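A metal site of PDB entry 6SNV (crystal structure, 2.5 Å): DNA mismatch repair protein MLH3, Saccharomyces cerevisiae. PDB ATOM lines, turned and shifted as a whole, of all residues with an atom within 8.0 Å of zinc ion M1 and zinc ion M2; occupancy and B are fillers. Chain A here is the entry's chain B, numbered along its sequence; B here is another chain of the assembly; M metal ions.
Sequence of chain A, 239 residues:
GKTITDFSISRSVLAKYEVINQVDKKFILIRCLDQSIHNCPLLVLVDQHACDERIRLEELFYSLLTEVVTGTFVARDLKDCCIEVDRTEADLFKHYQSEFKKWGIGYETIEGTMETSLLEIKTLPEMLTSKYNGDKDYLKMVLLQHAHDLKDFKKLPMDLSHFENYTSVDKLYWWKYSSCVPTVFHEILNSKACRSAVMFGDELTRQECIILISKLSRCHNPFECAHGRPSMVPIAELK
Ala 226 touches zinc ion M1 (N to ZN, 3.9 Å). The nearest printed residue that does not touch zinc ion M1 is His 49 (5.2 Å).
N of His 49 is in hydrogen-bond range of OD1 of Asp 47. The backbone carbonyl oxygen of Val 198 is in hydrogen-bond range of a ring nitrogen (ND1) of His 49 (2.7 Å). The side-chain sulfur (SG) of Cys 225 lies close to the backbone NH (N) of Arg 229, 3.3 Å away. A ring nitrogen (ND1) of His 227 sits close to the side-chain carboxylate (OE2) of Glu 53 (3.4 Å). NE of Arg 229 lies within salt-bridge range of OXT of Cys 265 of chain B (3.6 Å). N of His 227 sits close to SG of Cys 225, at 3.6 Å. N of Ala 226 sits close to OE2 of Glu 53. O of Cys 225 lies within hydrogen-bond range of NH1 of Arg 54 (3.2 Å).
The side-chain sulfur (SG) of Cys 265 of chain B binds zinc ion M1 (2.4 Å). Zinc ion M1 is bound by the side-chain carboxylate (OE2) of Glu 53, 2.4 Å away. The side-chain sulfur (SG) of Cys 225 is bound to zinc ion M1 (2.8 Å). Zinc ion M1 has three donor atoms within binding distance. Slightly farther from zinc ion M1 lies ND1 of His 227 (2.6 Å).
Zinc ion M2 is bound by OE1 of Glu 53 (1.9 Å), SG of Cys 265 of chain B (2.2 Å), NE2 of His 49 (2.2 Å) and SG of Cys 194 (2.4 Å). Zinc ion M2 has four donor atoms within binding distance.
Of the 23 residues printed, 4 come within 4 Å of zinc ion M2.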
ATOM      1  N   ASP A  47      -7.153 -11.034  12.565  1.00  0.00           N
ATOM      2  CA  ASP A  47      -8.592 -10.764  12.518  1.00  0.00           C
ATOM      3  C   ASP A  47      -9.059 -10.677  13.992  1.00  0.00           C
ATOM      4  O   ASP A  47      -8.937 -11.653  14.733  1.00  0.00           O
ATOM      5  CB  ASP A  47      -9.306 -11.896  11.755  1.00  0.00           C
ATOM      6  CG  ASP A  47     -10.828 -11.910  11.779  1.00  0.00           C
ATOM      7  OD1 ASP A  47     -11.426 -10.999  12.375  1.00  0.00           O
ATOM      8  OD2 ASP A  47     -11.419 -12.858  11.216  1.00  0.00           O
ATOM      9  N   HIS A  49     -12.060 -10.394  15.375  1.00  0.00           N
ATOM     10  CA  HIS A  49     -13.205 -11.229  15.709  1.00  0.00           C
ATOM     11  C   HIS A  49     -12.757 -12.670  15.955  1.00  0.00           C
ATOM     12  O   HIS A  49     -13.081 -13.230  17.000  1.00  0.00           O
ATOM     13  CB  HIS A  49     -14.302 -11.148  14.639  1.00  0.00           C
ATOM     14  CG  HIS A  49     -15.429 -12.103  14.884  1.00  0.00           C
ATOM     15  ND1 HIS A  49     -16.375 -11.868  15.857  1.00  0.00           N
ATOM     16  CD2 HIS A  49     -15.669 -13.300  14.311  1.00  0.00           C
ATOM     17  CE1 HIS A  49     -17.195 -12.909  15.812  1.00  0.00           C
ATOM     18  NE2 HIS A  49     -16.800 -13.802  14.909  1.00  0.00           N
ATOM     19  N   ALA A  50     -11.969 -13.235  14.999  1.00  0.00           N
ATOM     20  CA  ALA A  50     -11.402 -14.588  15.086  1.00  0.00           C
ATOM     21  C   ALA A  50     -10.514 -14.727  16.311  1.00  0.00           C
ATOM     22  O   ALA A  50     -10.577 -15.746  16.986  1.00  0.00           O
ATOM     23  CB  ALA A  50     -10.615 -14.899  13.835  1.00  0.00           C
ATOM     24  N   GLU A  53     -12.906 -14.613  19.480  1.00  0.00           N
ATOM     25  CA  GLU A  53     -13.669 -15.860  19.404  1.00  0.00           C
ATOM     26  C   GLU A  53     -12.813 -17.069  19.819  1.00  0.00           C
ATOM     27  O   GLU A  53     -13.301 -17.926  20.570  1.00  0.00           O
ATOM     28  CB  GLU A  53     -14.236 -16.047  17.993  1.00  0.00           C
ATOM     29  CG  GLU A  53     -14.901 -17.383  17.712  1.00  0.00           C
ATOM     30  CD  GLU A  53     -15.438 -17.430  16.306  1.00  0.00           C
ATOM     31  OE1 GLU A  53     -16.263 -16.552  15.955  1.00  0.00           O
ATOM     32  OE2 GLU A  53     -15.020 -18.319  15.542  1.00  0.00           O
ATOM     33  N   ARG A  54     -11.540 -17.123  19.372  1.00  0.00           N
ATOM     34  CA  ARG A  54     -10.615 -18.200  19.720  1.00  0.00           C
ATOM     35  C   ARG A  54     -10.316 -18.244  21.214  1.00  0.00           C
ATOM     36  O   ARG A  54     -10.298 -19.330  21.774  1.00  0.00           O
ATOM     37  CB  ARG A  54      -9.312 -18.089  18.927  1.00  0.00           C
ATOM     38  CG  ARG A  54      -8.414 -19.293  19.128  1.00  0.00           C
ATOM     39  CD  ARG A  54      -9.150 -20.491  18.629  1.00  0.00           C
ATOM     40  NE  ARG A  54      -8.752 -21.742  19.267  1.00  0.00           N
ATOM     41  CZ  ARG A  54      -9.089 -22.924  18.770  1.00  0.00           C
ATOM     42  NH1 ARG A  54      -9.773 -23.005  17.635  1.00  0.00           N
ATOM     43  NH2 ARG A  54      -8.719 -24.030  19.397  1.00  0.00           N
ATOM     44  N   ASN A 190     -19.207 -23.063  19.925  1.00  0.00           N
ATOM     45  CA  ASN A 190     -18.711 -22.301  18.784  1.00  0.00           C
ATOM     46  C   ASN A 190     -19.584 -21.050  18.621  1.00  0.00           C
ATOM     47  O   ASN A 190     -19.047 -19.952  18.433  1.00  0.00           O
ATOM     48  CB  ASN A 190     -18.840 -23.131  17.495  1.00  0.00           C
ATOM     49  CG  ASN A 190     -17.773 -24.157  17.221  1.00  0.00           C
ATOM     50  OD1 ASN A 190     -16.867 -24.426  18.026  1.00  0.00           O
ATOM     51  ND2 ASN A 190     -17.868 -24.766  16.045  1.00  0.00           N
ATOM     52  N   SER A 191     -20.920 -21.236  18.695  1.00  0.00           N
ATOM     53  CA  SER A 191     -21.952 -20.201  18.576  1.00  0.00           C
ATOM     54  C   SER A 191     -21.859 -19.192  19.724  1.00  0.00           C
ATOM     55  O   SER A 191     -22.022 -17.988  19.483  1.00  0.00           O
ATOM     56  CB  SER A 191     -23.336 -20.846  18.542  1.00  0.00           C
ATOM     57  OG  SER A 191     -24.402 -19.906  18.658  1.00  0.00           O
ATOM     58  N   ALA A 193     -19.133 -18.558  21.582  1.00  0.00           N
ATOM     59  CA  ALA A 193     -17.866 -17.869  21.362  1.00  0.00           C
ATOM     60  C   ALA A 193     -18.034 -16.780  20.311  1.00  0.00           C
ATOM     61  O   ALA A 193     -17.703 -15.622  20.578  1.00  0.00           O
ATOM     62  CB  ALA A 193     -16.785 -18.866  20.936  1.00  0.00           C
ATOM     63  N   CYS A 194     -18.645 -17.129  19.156  1.00  0.00           N
ATOM     64  CA  CYS A 194     -18.886 -16.216  18.033  1.00  0.00           C
ATOM     65  C   CYS A 194     -19.730 -14.999  18.409  1.00  0.00           C
ATOM     66  O   CYS A 194     -19.388 -13.881  18.045  1.00  0.00           O
ATOM     67  CB  CYS A 194     -19.463 -16.967  16.843  1.00  0.00           C
ATOM     68  SG  CYS A 194     -19.592 -15.977  15.330  1.00  0.00           S
ATOM     69  N   ARG A 195     -20.834 -15.225  19.140  1.00  0.00           N
ATOM     70  CA  ARG A 195     -21.771 -14.185  19.576  1.00  0.00           C
ATOM     71  C   ARG A 195     -21.226 -13.233  20.614  1.00  0.00           C
ATOM     72  O   ARG A 195     -21.610 -12.060  20.619  1.00  0.00           O
ATOM     73  CB  ARG A 195     -23.070 -14.806  20.087  1.00  0.00           C
ATOM     74  CG  ARG A 195     -24.000 -15.201  18.985  1.00  0.00           C
ATOM     75  CD  ARG A 195     -24.817 -14.045  18.418  1.00  0.00           C
ATOM     76  NE  ARG A 195     -25.797 -14.602  17.503  1.00  0.00           N
ATOM     77  CZ  ARG A 195     -27.021 -14.977  17.854  1.00  0.00           C
ATOM     78  NH1 ARG A 195     -27.467 -14.760  19.084  1.00  0.00           N
ATOM     79  NH2 ARG A 195     -27.824 -15.552  16.967  1.00  0.00           N
ATOM     80  N   SER A 196     -20.379 -13.738  21.528  1.00  0.00           N
ATOM     81  CA  SER A 196     -19.775 -12.977  22.606  1.00  0.00           C
ATOM     82  C   SER A 196     -18.520 -12.219  22.155  1.00  0.00           C
ATOM     83  O   SER A 196     -18.081 -11.299  22.850  1.00  0.00           O
ATOM     84  CB  SER A 196     -19.445 -13.891  23.773  1.00  0.00           C
ATOM     85  OG  SER A 196     -20.632 -14.430  24.315  1.00  0.00           O
ATOM     86  N   ALA A 197     -17.944 -12.617  20.990  1.00  0.00           N
ATOM     87  CA  ALA A 197     -16.728 -12.052  20.406  1.00  0.00           C
ATOM     88  C   ALA A 197     -16.940 -10.658  19.853  1.00  0.00           C
ATOM     89  O   ALA A 197     -18.063 -10.310  19.472  1.00  0.00           O
ATOM     90  CB  ALA A 197     -16.179 -12.960  19.312  1.00  0.00           C
ATOM     91  N   VAL A 198     -15.852  -9.872  19.825  1.00  0.00           N
ATOM     92  CA  VAL A 198     -15.787  -8.509  19.294  1.00  0.00           C
ATOM     93  C   VAL A 198     -16.023  -8.563  17.777  1.00  0.00           C
ATOM     94  O   VAL A 198     -15.651  -9.558  17.148  1.00  0.00           O
ATOM     95  CB  VAL A 198     -14.447  -7.803  19.731  1.00  0.00           C
ATOM     96  CG1 VAL A 198     -13.217  -8.310  18.964  1.00  0.00           C
ATOM     97  CG2 VAL A 198     -14.555  -6.290  19.670  1.00  0.00           C
ATOM     98  N   MET A 199     -16.656  -7.545  17.190  1.00  0.00           N
ATOM     99  CA  MET A 199     -16.954  -7.572  15.757  1.00  0.00           C
ATOM    100  C   MET A 199     -16.146  -6.597  14.902  1.00  0.00           C
ATOM    101  O   MET A 199     -15.445  -5.733  15.440  1.00  0.00           O
ATOM    102  CB  MET A 199     -18.438  -7.318  15.543  1.00  0.00           C
ATOM    103  CG  MET A 199     -19.218  -8.549  15.168  1.00  0.00           C
ATOM    104  SD  MET A 199     -20.973  -8.200  14.861  1.00  0.00           S
ATOM    105  CE  MET A 199     -20.861  -7.153  13.330  1.00  0.00           C
ATOM    106  N   GLU A 224      -6.432 -20.282  14.259  1.00  0.00           N
ATOM    107  CA  GLU A 224      -7.757 -20.437  13.641  1.00  0.00           C
ATOM    108  C   GLU A 224      -8.889 -20.079  14.574  1.00  0.00           C
ATOM    109  O   GLU A 224      -8.745 -20.227  15.790  1.00  0.00           O
ATOM    110  CB  GLU A 224      -7.958 -21.830  13.009  1.00  0.00           C
ATOM    111  CG  GLU A 224      -8.104 -22.964  13.992  1.00  0.00           C
ATOM    112  CD  GLU A 224      -8.517 -24.273  13.372  1.00  0.00           C
ATOM    113  OE1 GLU A 224      -7.875 -24.695  12.374  1.00  0.00           O
ATOM    114  OE2 GLU A 224      -9.488 -24.888  13.881  1.00  0.00           O
ATOM    115  N   CYS A 225     -10.026 -19.621  14.022  1.00  0.00           N
ATOM    116  CA  CYS A 225     -11.243 -19.263  14.750  1.00  0.00           C
ATOM    117  C   CYS A 225     -11.946 -20.539  15.262  1.00  0.00           C
ATOM    118  O   CYS A 225     -11.363 -21.627  15.202  1.00  0.00           O
ATOM    119  CB  CYS A 225     -12.165 -18.425  13.865  1.00  0.00           C
ATOM    120  SG  CYS A 225     -12.844 -19.329  12.444  1.00  0.00           S
ATOM    121  N   ALA A 226     -13.195 -20.424  15.757  1.00  0.00           N
ATOM    122  CA  ALA A 226     -13.953 -21.588  16.231  1.00  0.00           C
ATOM    123  C   ALA A 226     -14.346 -22.512  15.072  1.00  0.00           C
ATOM    124  O   ALA A 226     -14.196 -23.740  15.174  1.00  0.00           O
ATOM    125  CB  ALA A 226     -15.188 -21.139  17.009  1.00  0.00           C
ATOM    126  N   HIS A 227     -14.777 -21.920  13.937  1.00  0.00           N
ATOM    127  CA  HIS A 227     -15.245 -22.591  12.728  1.00  0.00           C
ATOM    128  C   HIS A 227     -14.110 -23.041  11.767  1.00  0.00           C
ATOM    129  O   HIS A 227     -14.374 -23.276  10.586  1.00  0.00           O
ATOM    130  CB  HIS A 227     -16.279 -21.697  12.001  1.00  0.00           C
ATOM    131  CG  HIS A 227     -17.419 -21.262  12.873  1.00  0.00           C
ATOM    132  ND1 HIS A 227     -17.282 -20.227  13.787  1.00  0.00           N
ATOM    133  CD2 HIS A 227     -18.672 -21.758  12.967  1.00  0.00           C
ATOM    134  CE1 HIS A 227     -18.457 -20.121  14.396  1.00  0.00           C
ATOM    135  NE2 HIS A 227     -19.327 -21.016  13.941  1.00  0.00           N
ATOM    136  N   GLY A 228     -12.908 -23.212  12.299  1.00  0.00           N
ATOM    137  CA  GLY A 228     -11.730 -23.690  11.576  1.00  0.00           C
ATOM    138  C   GLY A 228     -11.158 -22.859  10.439  1.00  0.00           C
ATOM    139  O   GLY A 228     -10.451 -23.407   9.589  1.00  0.00           O
ATOM    140  N   ARG A 229     -11.415 -21.532  10.422  1.00  0.00           N
ATOM    141  CA  ARG A 229     -10.877 -20.605   9.406  1.00  0.00           C
ATOM    142  C   ARG A 229      -9.695 -19.821  10.003  1.00  0.00           C
ATOM    143  O   ARG A 229      -9.689 -19.652  11.232  1.00  0.00           O
ATOM    144  CB  ARG A 229     -11.974 -19.661   8.892  1.00  0.00           C
ATOM    145  CG  ARG A 229     -13.092 -20.422   8.231  1.00  0.00           C
ATOM    146  CD  ARG A 229     -14.134 -19.500   7.643  1.00  0.00           C
ATOM    147  NE  ARG A 229     -15.264 -20.233   7.082  1.00  0.00           N
ATOM    148  CZ  ARG A 229     -15.338 -20.640   5.822  1.00  0.00           C
ATOM    149  NH1 ARG A 229     -14.345 -20.389   4.977  1.00  0.00           N
ATOM    150  NH2 ARG A 229     -16.412 -21.293   5.396  1.00  0.00           N
ATOM    151  N   PRO A 230      -8.676 -19.372   9.223  1.00  0.00           N
ATOM    152  CA  PRO A 230      -7.523 -18.677   9.833  1.00  0.00           C
ATOM    153  C   PRO A 230      -7.868 -17.406  10.595  1.00  0.00           C
ATOM    154  O   PRO A 230      -8.782 -16.678  10.203  1.00  0.00           O
ATOM    155  CB  PRO A 230      -6.598 -18.374   8.652  1.00  0.00           C
ATOM    156  CG  PRO A 230      -7.495 -18.400   7.460  1.00  0.00           C
ATOM    157  CD  PRO A 230      -8.493 -19.472   7.759  1.00  0.00           C
ATOM    158  N   ARG B 264     -16.581 -14.735   5.598  1.00  0.00           N
ATOM    159  CA  ARG B 264     -17.495 -15.655   6.279  1.00  0.00           C
ATOM    160  C   ARG B 264     -16.708 -16.274   7.429  1.00  0.00           C
ATOM    161  O   ARG B 264     -15.668 -16.890   7.209  1.00  0.00           O
ATOM    162  CB  ARG B 264     -18.047 -16.723   5.313  1.00  0.00           C
ATOM    163  CG  ARG B 264     -18.999 -16.148   4.265  1.00  0.00           C
ATOM    164  CD  ARG B 264     -19.705 -17.215   3.451  1.00  0.00           C
ATOM    165  NE  ARG B 264     -20.653 -16.625   2.502  1.00  0.00           N
ATOM    166  CZ  ARG B 264     -21.546 -17.318   1.814  1.00  0.00           C
ATOM    167  NH1 ARG B 264     -22.362 -16.693   0.976  1.00  0.00           N
ATOM    168  NH2 ARG B 264     -21.640 -18.638   1.945  1.00  0.00           N
ATOM    169  N   CYS B 265     -17.171 -16.031   8.659  1.00  0.00           N
ATOM    170  CA  CYS B 265     -16.525 -16.542   9.868  1.00  0.00           C
ATOM    171  C   CYS B 265     -16.860 -18.025  10.098  1.00  0.00           C
ATOM    172  O   CYS B 265     -18.061 -18.378  10.107  1.00  0.00           O
ATOM    173  CB  CYS B 265     -16.892 -15.684  11.080  1.00  0.00           C
ATOM    174  SG  CYS B 265     -16.323 -16.374  12.648  1.00  0.00           S
ATOM    175  OXT CYS B 265     -15.915 -18.815  10.289  1.00  0.00           O
HETATM  176 ZN    ZN M   1     -15.393 -18.493  13.155  1.00  0.00          ZN
HETATM  177 ZN    ZN M   2     -17.308 -15.923  14.531  1.00  0.00          ZN
